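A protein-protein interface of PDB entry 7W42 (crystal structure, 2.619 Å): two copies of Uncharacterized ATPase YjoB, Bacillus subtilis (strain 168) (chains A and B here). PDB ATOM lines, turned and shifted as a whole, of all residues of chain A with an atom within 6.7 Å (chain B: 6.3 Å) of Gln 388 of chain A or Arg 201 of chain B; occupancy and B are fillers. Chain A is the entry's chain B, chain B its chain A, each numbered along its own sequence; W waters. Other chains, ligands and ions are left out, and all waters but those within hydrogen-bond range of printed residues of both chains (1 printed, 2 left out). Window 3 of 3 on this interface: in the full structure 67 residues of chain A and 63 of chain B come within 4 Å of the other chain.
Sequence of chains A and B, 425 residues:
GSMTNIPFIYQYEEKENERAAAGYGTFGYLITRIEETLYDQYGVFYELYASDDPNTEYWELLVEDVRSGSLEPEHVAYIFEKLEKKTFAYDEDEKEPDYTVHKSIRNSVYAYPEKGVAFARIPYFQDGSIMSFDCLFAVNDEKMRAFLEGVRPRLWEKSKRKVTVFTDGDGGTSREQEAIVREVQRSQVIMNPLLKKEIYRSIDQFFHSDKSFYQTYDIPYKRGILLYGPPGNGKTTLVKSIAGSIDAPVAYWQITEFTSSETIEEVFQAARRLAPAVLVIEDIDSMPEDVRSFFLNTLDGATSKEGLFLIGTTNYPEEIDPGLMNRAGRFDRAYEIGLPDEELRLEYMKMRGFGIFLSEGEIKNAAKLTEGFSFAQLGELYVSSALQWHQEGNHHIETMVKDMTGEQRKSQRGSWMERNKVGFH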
ATOM      1  N   VAL A 383     -21.649 -23.932  17.756  1.00  0.00           N
ATOM      2  CA  VAL A 383     -22.183 -25.039  18.543  1.00  0.00           C
ATOM      3  C   VAL A 383     -21.866 -24.865  20.026  1.00  0.00           C
ATOM      4  O   VAL A 383     -22.699 -25.156  20.892  1.00  0.00           O
ATOM      5  CB  VAL A 383     -21.631 -26.377  18.017  1.00  0.00           C
ATOM      6  CG1 VAL A 383     -22.208 -27.515  18.815  1.00  0.00           C
ATOM      7  CG2 VAL A 383     -21.945 -26.523  16.550  1.00  0.00           C
ATOM      8  N   SER A 384     -20.648 -24.430  20.346  1.00  0.00           N
ATOM      9  CA  SER A 384     -20.238 -24.394  21.746  1.00  0.00           C
ATOM     10  C   SER A 384     -20.931 -23.262  22.488  1.00  0.00           C
ATOM     11  O   SER A 384     -21.386 -23.452  23.615  1.00  0.00           O
ATOM     12  CB  SER A 384     -18.723 -24.253  21.840  1.00  0.00           C
ATOM     13  OG  SER A 384     -18.106 -25.309  21.125  1.00  0.00           O
ATOM     14  N   SER A 385     -21.015 -22.077  21.868  1.00  0.00           N
ATOM     15  CA  SER A 385     -21.810 -20.995  22.434  1.00  0.00           C
ATOM     16  C   SER A 385     -23.253 -21.424  22.627  1.00  0.00           C
ATOM     17  O   SER A 385     -23.801 -21.301  23.726  1.00  0.00           O
ATOM     18  CB  SER A 385     -21.763 -19.771  21.527  1.00  0.00           C
ATOM     19  OG  SER A 385     -20.433 -19.448  21.204  1.00  0.00           O
ATOM     20  N   ALA A 386     -23.885 -21.922  21.550  1.00  0.00           N
ATOM     21  CA  ALA A 386     -25.291 -22.321  21.586  1.00  0.00           C
ATOM     22  C   ALA A 386     -25.560 -23.316  22.701  1.00  0.00           C
ATOM     23  O   ALA A 386     -26.545 -23.181  23.426  1.00  0.00           O
ATOM     24  CB  ALA A 386     -25.709 -22.907  20.241  1.00  0.00           C
ATOM     25  N   LEU A 387     -24.681 -24.308  22.872  1.00  0.00           N
ATOM     26  CA  LEU A 387     -24.836 -25.242  23.983  1.00  0.00           C
ATOM     27  C   LEU A 387     -24.832 -24.509  25.314  1.00  0.00           C
ATOM     28  O   LEU A 387     -25.685 -24.757  26.174  1.00  0.00           O
ATOM     29  CB  LEU A 387     -23.723 -26.277  23.969  1.00  0.00           C
ATOM     30  CG  LEU A 387     -23.866 -27.447  23.014  1.00  0.00           C
ATOM     31  CD1 LEU A 387     -22.498 -28.096  22.847  1.00  0.00           C
ATOM     32  CD2 LEU A 387     -24.890 -28.423  23.556  1.00  0.00           C
ATOM     33  N   GLN A 388     -23.859 -23.611  25.503  1.00  0.00           N
ATOM     34  CA  GLN A 388     -23.785 -22.826  26.729  1.00  0.00           C
ATOM     35  C   GLN A 388     -25.048 -21.993  26.917  1.00  0.00           C
ATOM     36  O   GLN A 388     -25.636 -21.960  28.004  1.00  0.00           O
ATOM     37  CB  GLN A 388     -22.549 -21.930  26.688  1.00  0.00           C
ATOM     38  CG  GLN A 388     -22.003 -21.567  28.062  1.00  0.00           C
ATOM     39  CD  GLN A 388     -20.894 -22.502  28.504  1.00  0.00           C
ATOM     40  OE1 GLN A 388     -20.171 -23.058  27.672  1.00  0.00           O
ATOM     41  NE2 GLN A 388     -20.749 -22.677  29.821  1.00  0.00           N
ATOM     42  N   TRP A 389     -25.478 -21.315  25.859  1.00  0.00           N
ATOM     43  CA  TRP A 389     -26.688 -20.518  25.939  1.00  0.00           C
ATOM     44  C   TRP A 389     -27.887 -21.384  26.314  1.00  0.00           C
ATOM     45  O   TRP A 389     -28.608 -21.102  27.282  1.00  0.00           O
ATOM     46  CB  TRP A 389     -26.894 -19.845  24.602  1.00  0.00           C
ATOM     47  CG  TRP A 389     -28.115 -19.070  24.486  1.00  0.00           C
ATOM     48  CD1 TRP A 389     -29.194 -19.361  23.714  1.00  0.00           C
ATOM     49  CD2 TRP A 389     -28.393 -17.828  25.120  1.00  0.00           C
ATOM     50  NE1 TRP A 389     -30.130 -18.375  23.820  1.00  0.00           N
ATOM     51  CE2 TRP A 389     -29.666 -17.417  24.682  1.00  0.00           C
ATOM     52  CE3 TRP A 389     -27.686 -17.009  26.006  1.00  0.00           C
ATOM     53  CZ2 TRP A 389     -30.261 -16.226  25.113  1.00  0.00           C
ATOM     54  CZ3 TRP A 389     -28.276 -15.818  26.432  1.00  0.00           C
ATOM     55  CH2 TRP A 389     -29.553 -15.443  25.986  1.00  0.00           C
ATOM     56  N   HIS A 390     -28.078 -22.480  25.585  1.00  0.00           N
ATOM     57  CA  HIS A 390     -29.232 -23.335  25.804  1.00  0.00           C
ATOM     58  C   HIS A 390     -29.246 -23.936  27.212  1.00  0.00           C
ATOM     59  O   HIS A 390     -30.305 -24.039  27.834  1.00  0.00           O
ATOM     60  CB  HIS A 390     -29.245 -24.422  24.729  1.00  0.00           C
ATOM     61  CG  HIS A 390     -30.416 -25.346  24.812  1.00  0.00           C
ATOM     62  ND1 HIS A 390     -31.689 -24.974  24.420  1.00  0.00           N
ATOM     63  CD2 HIS A 390     -30.506 -26.632  25.229  1.00  0.00           C
ATOM     64  CE1 HIS A 390     -32.512 -25.993  24.587  1.00  0.00           C
ATOM     65  NE2 HIS A 390     -31.821 -27.009  25.085  1.00  0.00           N
ATOM     66  N   GLN A 391     -28.091 -24.340  27.733  1.00  0.00           N
ATOM     67  CA  GLN A 391     -28.095 -25.109  28.974  1.00  0.00           C
ATOM     68  C   GLN A 391     -27.967 -24.240  30.221  1.00  0.00           C
ATOM     69  O   GLN A 391     -28.441 -24.637  31.289  1.00  0.00           O
ATOM     70  CB  GLN A 391     -26.970 -26.154  28.966  1.00  0.00           C
ATOM     71  CG  GLN A 391     -27.069 -27.164  27.828  1.00  0.00           C
ATOM     72  CD  GLN A 391     -25.956 -28.211  27.840  1.00  0.00           C
ATOM     73  OE1 GLN A 391     -25.124 -28.246  28.742  1.00  0.00           O
ATOM     74  NE2 GLN A 391     -25.962 -29.081  26.846  1.00  0.00           N
ATOM     75  N   GLU A 392     -27.359 -23.060  30.109  1.00  0.00           N
ATOM     76  CA  GLU A 392     -27.050 -22.229  31.265  1.00  0.00           C
ATOM     77  C   GLU A 392     -27.529 -20.790  31.149  1.00  0.00           C
ATOM     78  O   GLU A 392     -27.381 -20.030  32.109  1.00  0.00           O
ATOM     79  CB  GLU A 392     -25.535 -22.207  31.522  1.00  0.00           C
ATOM     80  CG  GLU A 392     -24.979 -23.498  32.078  1.00  0.00           C
ATOM     81  CD  GLU A 392     -23.533 -23.680  31.679  1.00  0.00           C
ATOM     82  OE1 GLU A 392     -22.839 -22.651  31.499  1.00  0.00           O
ATOM     83  OE2 GLU A 392     -23.096 -24.840  31.515  1.00  0.00           O
ATOM     84  N   GLY A 393     -28.064 -20.379  30.017  1.00  0.00           N
ATOM     85  CA  GLY A 393     -28.635 -19.066  29.987  1.00  0.00           C
ATOM     86  C   GLY A 393     -27.657 -17.954  29.745  1.00  0.00           C
ATOM     87  O   GLY A 393     -28.047 -16.786  29.848  1.00  0.00           O
ATOM     88  N   ASN A 394     -26.400 -18.265  29.432  1.00  0.00           N
ATOM     89  CA  ASN A 394     -25.510 -17.265  28.858  1.00  0.00           C
ATOM     90  C   ASN A 394     -24.424 -17.963  28.050  1.00  0.00           C
ATOM     91  O   ASN A 394     -24.109 -19.131  28.278  1.00  0.00           O
ATOM     92  CB  ASN A 394     -24.914 -16.331  29.925  1.00  0.00           C
ATOM     93  CG  ASN A 394     -24.126 -17.065  30.970  1.00  0.00           C
ATOM     94  OD1 ASN A 394     -23.034 -17.566  30.699  1.00  0.00           O
ATOM     95  ND2 ASN A 394     -24.663 -17.116  32.190  1.00  0.00           N
ATOM     96  N   HIS A 395     -23.838 -17.215  27.110  1.00  0.00           N
ATOM     97  CA  HIS A 395     -23.044 -17.785  26.022  1.00  0.00           C
ATOM     98  C   HIS A 395     -21.545 -17.842  26.311  1.00  0.00           C
ATOM     99  O   HIS A 395     -20.878 -18.792  25.872  1.00  0.00           O
ATOM    100  CB  HIS A 395     -23.288 -16.984  24.740  1.00  0.00           C
ATOM    101  CG  HIS A 395     -23.341 -15.505  24.961  1.00  0.00           C
ATOM    102  ND1 HIS A 395     -22.206 -14.738  25.127  1.00  0.00           N
ATOM    103  CD2 HIS A 395     -24.389 -14.653  25.066  1.00  0.00           C
ATOM    104  CE1 HIS A 395     -22.553 -13.478  25.307  1.00  0.00           C
ATOM    105  NE2 HIS A 395     -23.872 -13.401  25.277  1.00  0.00           N
ATOM    106  N   HIS A 396     -20.994 -16.834  27.011  1.00  0.00           N
ATOM    107  CA  HIS A 396     -19.553 -16.762  27.321  1.00  0.00           C
ATOM    108  C   HIS A 396     -18.685 -16.682  26.064  1.00  0.00           C
ATOM    109  O   HIS A 396     -17.635 -17.326  25.981  1.00  0.00           O
ATOM    110  CB  HIS A 396     -19.098 -17.956  28.174  1.00  0.00           C
ATOM    111  CG  HIS A 396     -19.466 -17.858  29.621  1.00  0.00           C
ATOM    112  ND1 HIS A 396     -19.859 -18.953  30.367  1.00  0.00           N
ATOM    113  CD2 HIS A 396     -19.489 -16.799  30.465  1.00  0.00           C
ATOM    114  CE1 HIS A 396     -20.119 -18.568  31.603  1.00  0.00           C
ATOM    115  NE2 HIS A 396     -19.902 -17.266  31.689  1.00  0.00           N
ATOM    116  N   MET A 400     -14.849 -18.622  25.071  1.00  0.00           N
ATOM    117  CA  MET A 400     -14.768 -19.726  24.117  1.00  0.00           C
ATOM    118  C   MET A 400     -13.838 -19.393  22.959  1.00  0.00           C
ATOM    119  O   MET A 400     -13.151 -20.279  22.431  1.00  0.00           O
ATOM    120  CB  MET A 400     -16.162 -20.085  23.598  1.00  0.00           C
ATOM    121  CG  MET A 400     -17.150 -20.223  24.728  1.00  0.00           C
ATOM    122  SD  MET A 400     -18.160 -21.687  24.625  1.00  0.00           S
ATOM    123  CE  MET A 400     -16.944 -23.007  24.730  1.00  0.00           C
ATOM    124  N   ASP A 403     -10.551 -20.119  24.611  1.00  0.00           N
ATOM    125  CA  ASP A 403     -10.432 -21.578  24.713  1.00  0.00           C
ATOM    126  C   ASP A 403     -10.007 -22.213  23.393  1.00  0.00           C
ATOM    127  O   ASP A 403      -9.258 -23.197  23.381  1.00  0.00           O
ATOM    128  CB  ASP A 403     -11.757 -22.203  25.153  1.00  0.00           C
ATOM    129  CG  ASP A 403     -12.028 -22.057  26.638  1.00  0.00           C
ATOM    130  OD1 ASP A 403     -11.146 -21.560  27.380  1.00  0.00           O
ATOM    131  OD2 ASP A 403     -13.145 -22.443  27.058  1.00  0.00           O
ATOM    132  N   LEU B 194     -12.765 -29.105  34.550  1.00  0.00           N
ATOM    133  CA  LEU B 194     -13.265 -28.077  33.643  1.00  0.00           C
ATOM    134  C   LEU B 194     -13.529 -28.643  32.262  1.00  0.00           C
ATOM    135  O   LEU B 194     -14.435 -28.174  31.568  1.00  0.00           O
ATOM    136  CB  LEU B 194     -12.281 -26.914  33.571  1.00  0.00           C
ATOM    137  CG  LEU B 194     -12.575 -25.860  34.631  1.00  0.00           C
ATOM    138  CD1 LEU B 194     -11.290 -25.172  35.100  1.00  0.00           C
ATOM    139  CD2 LEU B 194     -13.584 -24.877  34.069  1.00  0.00           C
ATOM    140  N   LYS B 196     -14.051 -32.021  31.646  1.00  0.00           N
ATOM    141  CA  LYS B 196     -15.159 -32.942  31.842  1.00  0.00           C
ATOM    142  C   LYS B 196     -16.482 -32.225  31.673  1.00  0.00           C
ATOM    143  O   LYS B 196     -17.381 -32.712  30.986  1.00  0.00           O
ATOM    144  CB  LYS B 196     -15.050 -33.563  33.235  1.00  0.00           C
ATOM    145  CG  LYS B 196     -16.112 -34.568  33.612  1.00  0.00           C
ATOM    146  CD  LYS B 196     -15.963 -34.890  35.090  1.00  0.00           C
ATOM    147  CE  LYS B 196     -16.523 -36.218  35.484  1.00  0.00           C
ATOM    148  NZ  LYS B 196     -15.883 -36.522  36.795  1.00  0.00           N
ATOM    149  N   LYS B 197     -16.627 -31.078  32.332  1.00  0.00           N
ATOM    150  CA  LYS B 197     -17.841 -30.285  32.192  1.00  0.00           C
ATOM    151  C   LYS B 197     -18.105 -29.933  30.736  1.00  0.00           C
ATOM    152  O   LYS B 197     -19.250 -30.001  30.266  1.00  0.00           O
ATOM    153  CB  LYS B 197     -17.727 -29.012  33.031  1.00  0.00           C
ATOM    154  CG  LYS B 197     -19.047 -28.496  33.548  1.00  0.00           C
ATOM    155  CD  LYS B 197     -18.982 -26.999  33.882  1.00  0.00           C
ATOM    156  CE  LYS B 197     -20.387 -26.397  34.042  1.00  0.00           C
ATOM    157  NZ  LYS B 197     -20.372 -24.908  34.188  1.00  0.00           N
ATOM    158  N   GLU B 198     -17.054 -29.577  29.998  1.00  0.00           N
ATOM    159  CA  GLU B 198     -17.256 -29.083  28.643  1.00  0.00           C
ATOM    160  C   GLU B 198     -17.674 -30.206  27.713  1.00  0.00           C
ATOM    161  O   GLU B 198     -18.592 -30.038  26.904  1.00  0.00           O
ATOM    162  CB  GLU B 198     -15.989 -28.395  28.123  1.00  0.00           C
ATOM    163  CG  GLU B 198     -16.222 -27.544  26.865  1.00  0.00           C
ATOM    164  CD  GLU B 198     -15.056 -27.599  25.867  1.00  0.00           C
ATOM    165  OE1 GLU B 198     -15.291 -27.905  24.667  1.00  0.00           O
ATOM    166  OE2 GLU B 198     -13.902 -27.323  26.287  1.00  0.00           O
ATOM    167  N   ILE B 199     -17.014 -31.359  27.816  1.00  0.00           N
ATOM    168  CA  ILE B 199     -17.336 -32.470  26.931  1.00  0.00           C
ATOM    169  C   ILE B 199     -18.760 -32.933  27.181  1.00  0.00           C
ATOM    170  O   ILE B 199     -19.538 -33.139  26.244  1.00  0.00           O
ATOM    171  CB  ILE B 199     -16.321 -33.615  27.120  1.00  0.00           C
ATOM    172  CG1 ILE B 199     -14.923 -33.157  26.709  1.00  0.00           C
ATOM    173  CG2 ILE B 199     -16.699 -34.816  26.281  1.00  0.00           C
ATOM    174  CD1 ILE B 199     -13.904 -34.254  26.783  1.00  0.00           C
ATOM    175  N   TYR B 200     -19.134 -33.067  28.452  1.00  0.00           N
ATOM    176  CA  TYR B 200     -20.462 -33.546  28.793  1.00  0.00           C
ATOM    177  C   TYR B 200     -21.574 -32.593  28.379  1.00  0.00           C
ATOM    178  O   TYR B 200     -22.728 -33.014  28.339  1.00  0.00           O
ATOM    179  CB  TYR B 200     -20.536 -33.836  30.289  1.00  0.00           C
ATOM    180  CG  TYR B 200     -20.102 -35.253  30.585  1.00  0.00           C
ATOM    181  CD1 TYR B 200     -20.980 -36.322  30.431  1.00  0.00           C
ATOM    182  CD2 TYR B 200     -18.801 -35.529  30.958  1.00  0.00           C
ATOM    183  CE1 TYR B 200     -20.572 -37.621  30.681  1.00  0.00           C
ATOM    184  CE2 TYR B 200     -18.383 -36.810  31.212  1.00  0.00           C
ATOM    185  CZ  TYR B 200     -19.266 -37.854  31.077  1.00  0.00           C
ATOM    186  OH  TYR B 200     -18.828 -39.123  31.333  1.00  0.00           O
ATOM    187  N   ARG B 201     -21.276 -31.331  28.080  1.00  0.00           N
ATOM    188  CA  ARG B 201     -22.300 -30.474  27.488  1.00  0.00           C
ATOM    189  C   ARG B 201     -22.733 -31.033  26.141  1.00  0.00           C
ATOM    190  O   ARG B 201     -23.927 -31.100  25.837  1.00  0.00           O
ATOM    191  CB  ARG B 201     -21.787 -29.036  27.320  1.00  0.00           C
ATOM    192  CG  ARG B 201     -21.650 -28.210  28.592  1.00  0.00           C
ATOM    193  CD  ARG B 201     -21.426 -26.731  28.272  1.00  0.00           C
ATOM    194  NE  ARG B 201     -20.279 -26.206  29.014  1.00  0.00           N
ATOM    195  CZ  ARG B 201     -19.156 -25.728  28.465  1.00  0.00           C
ATOM    196  NH1 ARG B 201     -19.011 -25.663  27.143  1.00  0.00           N
ATOM    197  NH2 ARG B 201     -18.169 -25.289  29.241  1.00  0.00           N
ATOM    198  N   SER B 202     -21.767 -31.433  25.314  1.00  0.00           N
ATOM    199  CA  SER B 202     -22.080 -32.060  24.036  1.00  0.00           C
ATOM    200  C   SER B 202     -22.761 -33.401  24.247  1.00  0.00           C
ATOM    201  O   SER B 202     -23.752 -33.720  23.586  1.00  0.00           O
ATOM    202  CB  SER B 202     -20.797 -32.248  23.221  1.00  0.00           C
ATOM    203  OG  SER B 202     -20.356 -31.037  22.643  1.00  0.00           O
ATOM    204  N   ILE B 203     -22.221 -34.209  25.156  1.00  0.00           N
ATOM    205  CA  ILE B 203     -22.708 -35.568  25.323  1.00  0.00           C
ATOM    206  C   ILE B 203     -24.145 -35.553  25.812  1.00  0.00           C
ATOM    207  O   ILE B 203     -24.995 -36.270  25.286  1.00  0.00           O
ATOM    208  CB  ILE B 203     -21.804 -36.352  26.293  1.00  0.00           C
ATOM    209  CG1 ILE B 203     -20.423 -36.617  25.679  1.00  0.00           C
ATOM    210  CG2 ILE B 203     -22.509 -37.650  26.741  1.00  0.00           C
ATOM    211  CD1 ILE B 203     -19.449 -37.232  26.675  1.00  0.00           C
ATOM    212  N   ASP B 204     -24.433 -34.735  26.826  1.00  0.00           N
ATOM    213  CA  ASP B 204     -25.776 -34.706  27.390  1.00  0.00           C
ATOM    214  C   ASP B 204     -26.777 -34.189  26.376  1.00  0.00           C
ATOM    215  O   ASP B 204     -27.902 -34.693  26.303  1.00  0.00           O
ATOM    216  CB  ASP B 204     -25.807 -33.858  28.657  1.00  0.00           C
ATOM    217  CG  ASP B 204     -25.123 -34.539  29.825  1.00  0.00           C
ATOM    218  OD1 ASP B 204     -25.146 -35.798  29.867  1.00  0.00           O
ATOM    219  OD2 ASP B 204     -24.557 -33.824  30.691  1.00  0.00           O
ATOM    220  N   GLN B 205     -26.382 -33.207  25.565  1.00  0.00           N
ATOM    221  CA  GLN B 205     -27.292 -32.728  24.537  1.00  0.00           C
ATOM    222  C   GLN B 205     -27.526 -33.794  23.479  1.00  0.00           C
ATOM    223  O   GLN B 205     -28.647 -33.948  22.984  1.00  0.00           O
ATOM    224  CB  GLN B 205     -26.754 -31.464  23.891  1.00  0.00           C
ATOM    225  CG  GLN B 205     -27.849 -30.559  23.411  1.00  0.00           C
ATOM    226  CD  GLN B 205     -28.758 -30.098  24.554  1.00  0.00           C
ATOM    227  OE1 GLN B 205     -28.289 -29.541  25.556  1.00  0.00           O
ATOM    228  NE2 GLN B 205     -30.067 -30.344  24.411  1.00  0.00           N
ATOM    229  N   PHE B 206     -26.476 -34.537  23.127  1.00  0.00           N
ATOM    230  CA  PHE B 206     -26.549 -35.462  22.004  1.00  0.00           C
ATOM    231  C   PHE B 206     -27.339 -36.709  22.381  1.00  0.00           C
ATOM    232  O   PHE B 206     -28.088 -37.253  21.557  1.00  0.00           O
ATOM    233  CB  PHE B 206     -25.127 -35.818  21.549  1.00  0.00           C
ATOM    234  CG  PHE B 206     -25.042 -36.459  20.192  1.00  0.00           C
ATOM    235  CD1 PHE B 206     -25.117 -37.829  20.053  1.00  0.00           C
ATOM    236  CD2 PHE B 206     -24.826 -35.695  19.060  1.00  0.00           C
ATOM    237  CE1 PHE B 206     -25.014 -38.425  18.796  1.00  0.00           C
ATOM    238  CE2 PHE B 206     -24.729 -36.292  17.793  1.00  0.00           C
ATOM    239  CZ  PHE B 206     -24.818 -37.650  17.669  1.00  0.00           C
ATOM    240  N   TYR B 214     -30.844 -29.502  18.220  1.00  0.00           N
ATOM    241  CA  TYR B 214     -30.142 -29.520  16.940  1.00  0.00           C
ATOM    242  C   TYR B 214     -30.942 -28.834  15.846  1.00  0.00           C
ATOM    243  O   TYR B 214     -30.361 -28.181  14.977  1.00  0.00           O
ATOM    244  CB  TYR B 214     -29.771 -30.970  16.584  1.00  0.00           C
ATOM    245  CG  TYR B 214     -28.748 -31.425  17.574  1.00  0.00           C
ATOM    246  CD1 TYR B 214     -27.412 -31.088  17.408  1.00  0.00           C
ATOM    247  CD2 TYR B 214     -29.122 -32.042  18.750  1.00  0.00           C
ATOM    248  CE1 TYR B 214     -26.471 -31.421  18.349  1.00  0.00           C
ATOM    249  CE2 TYR B 214     -28.174 -32.382  19.696  1.00  0.00           C
ATOM    250  CZ  TYR B 214     -26.861 -32.065  19.483  1.00  0.00           C
ATOM    251  OH  TYR B 214     -25.916 -32.395  20.412  1.00  0.00           O
HETATM  252  O   HOH W   1     -32.775 -29.599  25.763  1.00  0.00           O
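Water W1 lies within hydrogen-bond range of a ring nitrogen (NE2) of His 390 of chain A and the side-chain amide nitrogen (NE2) of Gln 205 of chain B.
No position is printed for both chains.
Of the 8 pairs that touch across the chains among the printed residues, none has its exchanged pair printed and touching as well.
Hydrophobic or aromatic side chains of chain A that line the printed part of chain B: Leu 387 and His 390.
Printed residues of chain B that touch a printed residue of chain A: Lys 197, Arg 201, Ser 202 and Gln 205.
Among the printed residues, 8 pairs touch across the chains.
Among the printed residues, merely in contact across the chains: Leu 387 of chain A with Gln 205 of chain B (3.6 Å), Leu 387 of chain A with Ser 202 of chain B (3.6 Å), Leu 387 of chain A with Arg 201 of chain B (3.6 Å) and His 390 of chain A with Gln 205 of chain B (3.7 Å).
NZ of Lys 197 of chain B is in salt-bridge range of OE2 of Glu 392 of chain A.
NH1 of Arg 201 of chain B lies within hydrogen-bond range of OE1 of Gln 388 of chain A (2.9 Å).
The backbone carbonyl oxygen (O) of Arg 201 of chain B lies within hydrogen-bond range of the side-chain amide nitrogen (NE2) of Gln 391 of chain A (3.0 Å).
The side-chain amide oxygen (OE1) of Gln 205 of chain B lies within hydrogen-bond range of the side-chain amide nitrogen (NE2) of Gln 391 of chain A (2.7 Å).
NE2 of Gln 388 of chain A is in hydrogen-bond range of OE1 of Glu 392 of chain A, at 2.7 Å.
Gln 388 of chain A touches just one residue of chain B: Arg 201 (2.9 Å).
Of the printed residues of chain A, Arg 201 of chain B touches Leu 387 (3.6 Å), Gln 388 (2.9 Å) and Gln 391 (3.0 Å).
Of the printed residues of chain B, Leu 387 of chain A touches Arg 201 (3.6 Å), Ser 202 (3.6 Å) and Gln 205 (3.6 Å).
Printed residues of chain A within 4 Å of Gln 205 of chain B: Leu 387 (3.6 Å), His 390 (3.7 Å) and Gln 391 (2.7 Å).
The nearest printed residue of chain B that does not touch Leu 387 of chain A is Tyr 214 of chain B (5.2 Å).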
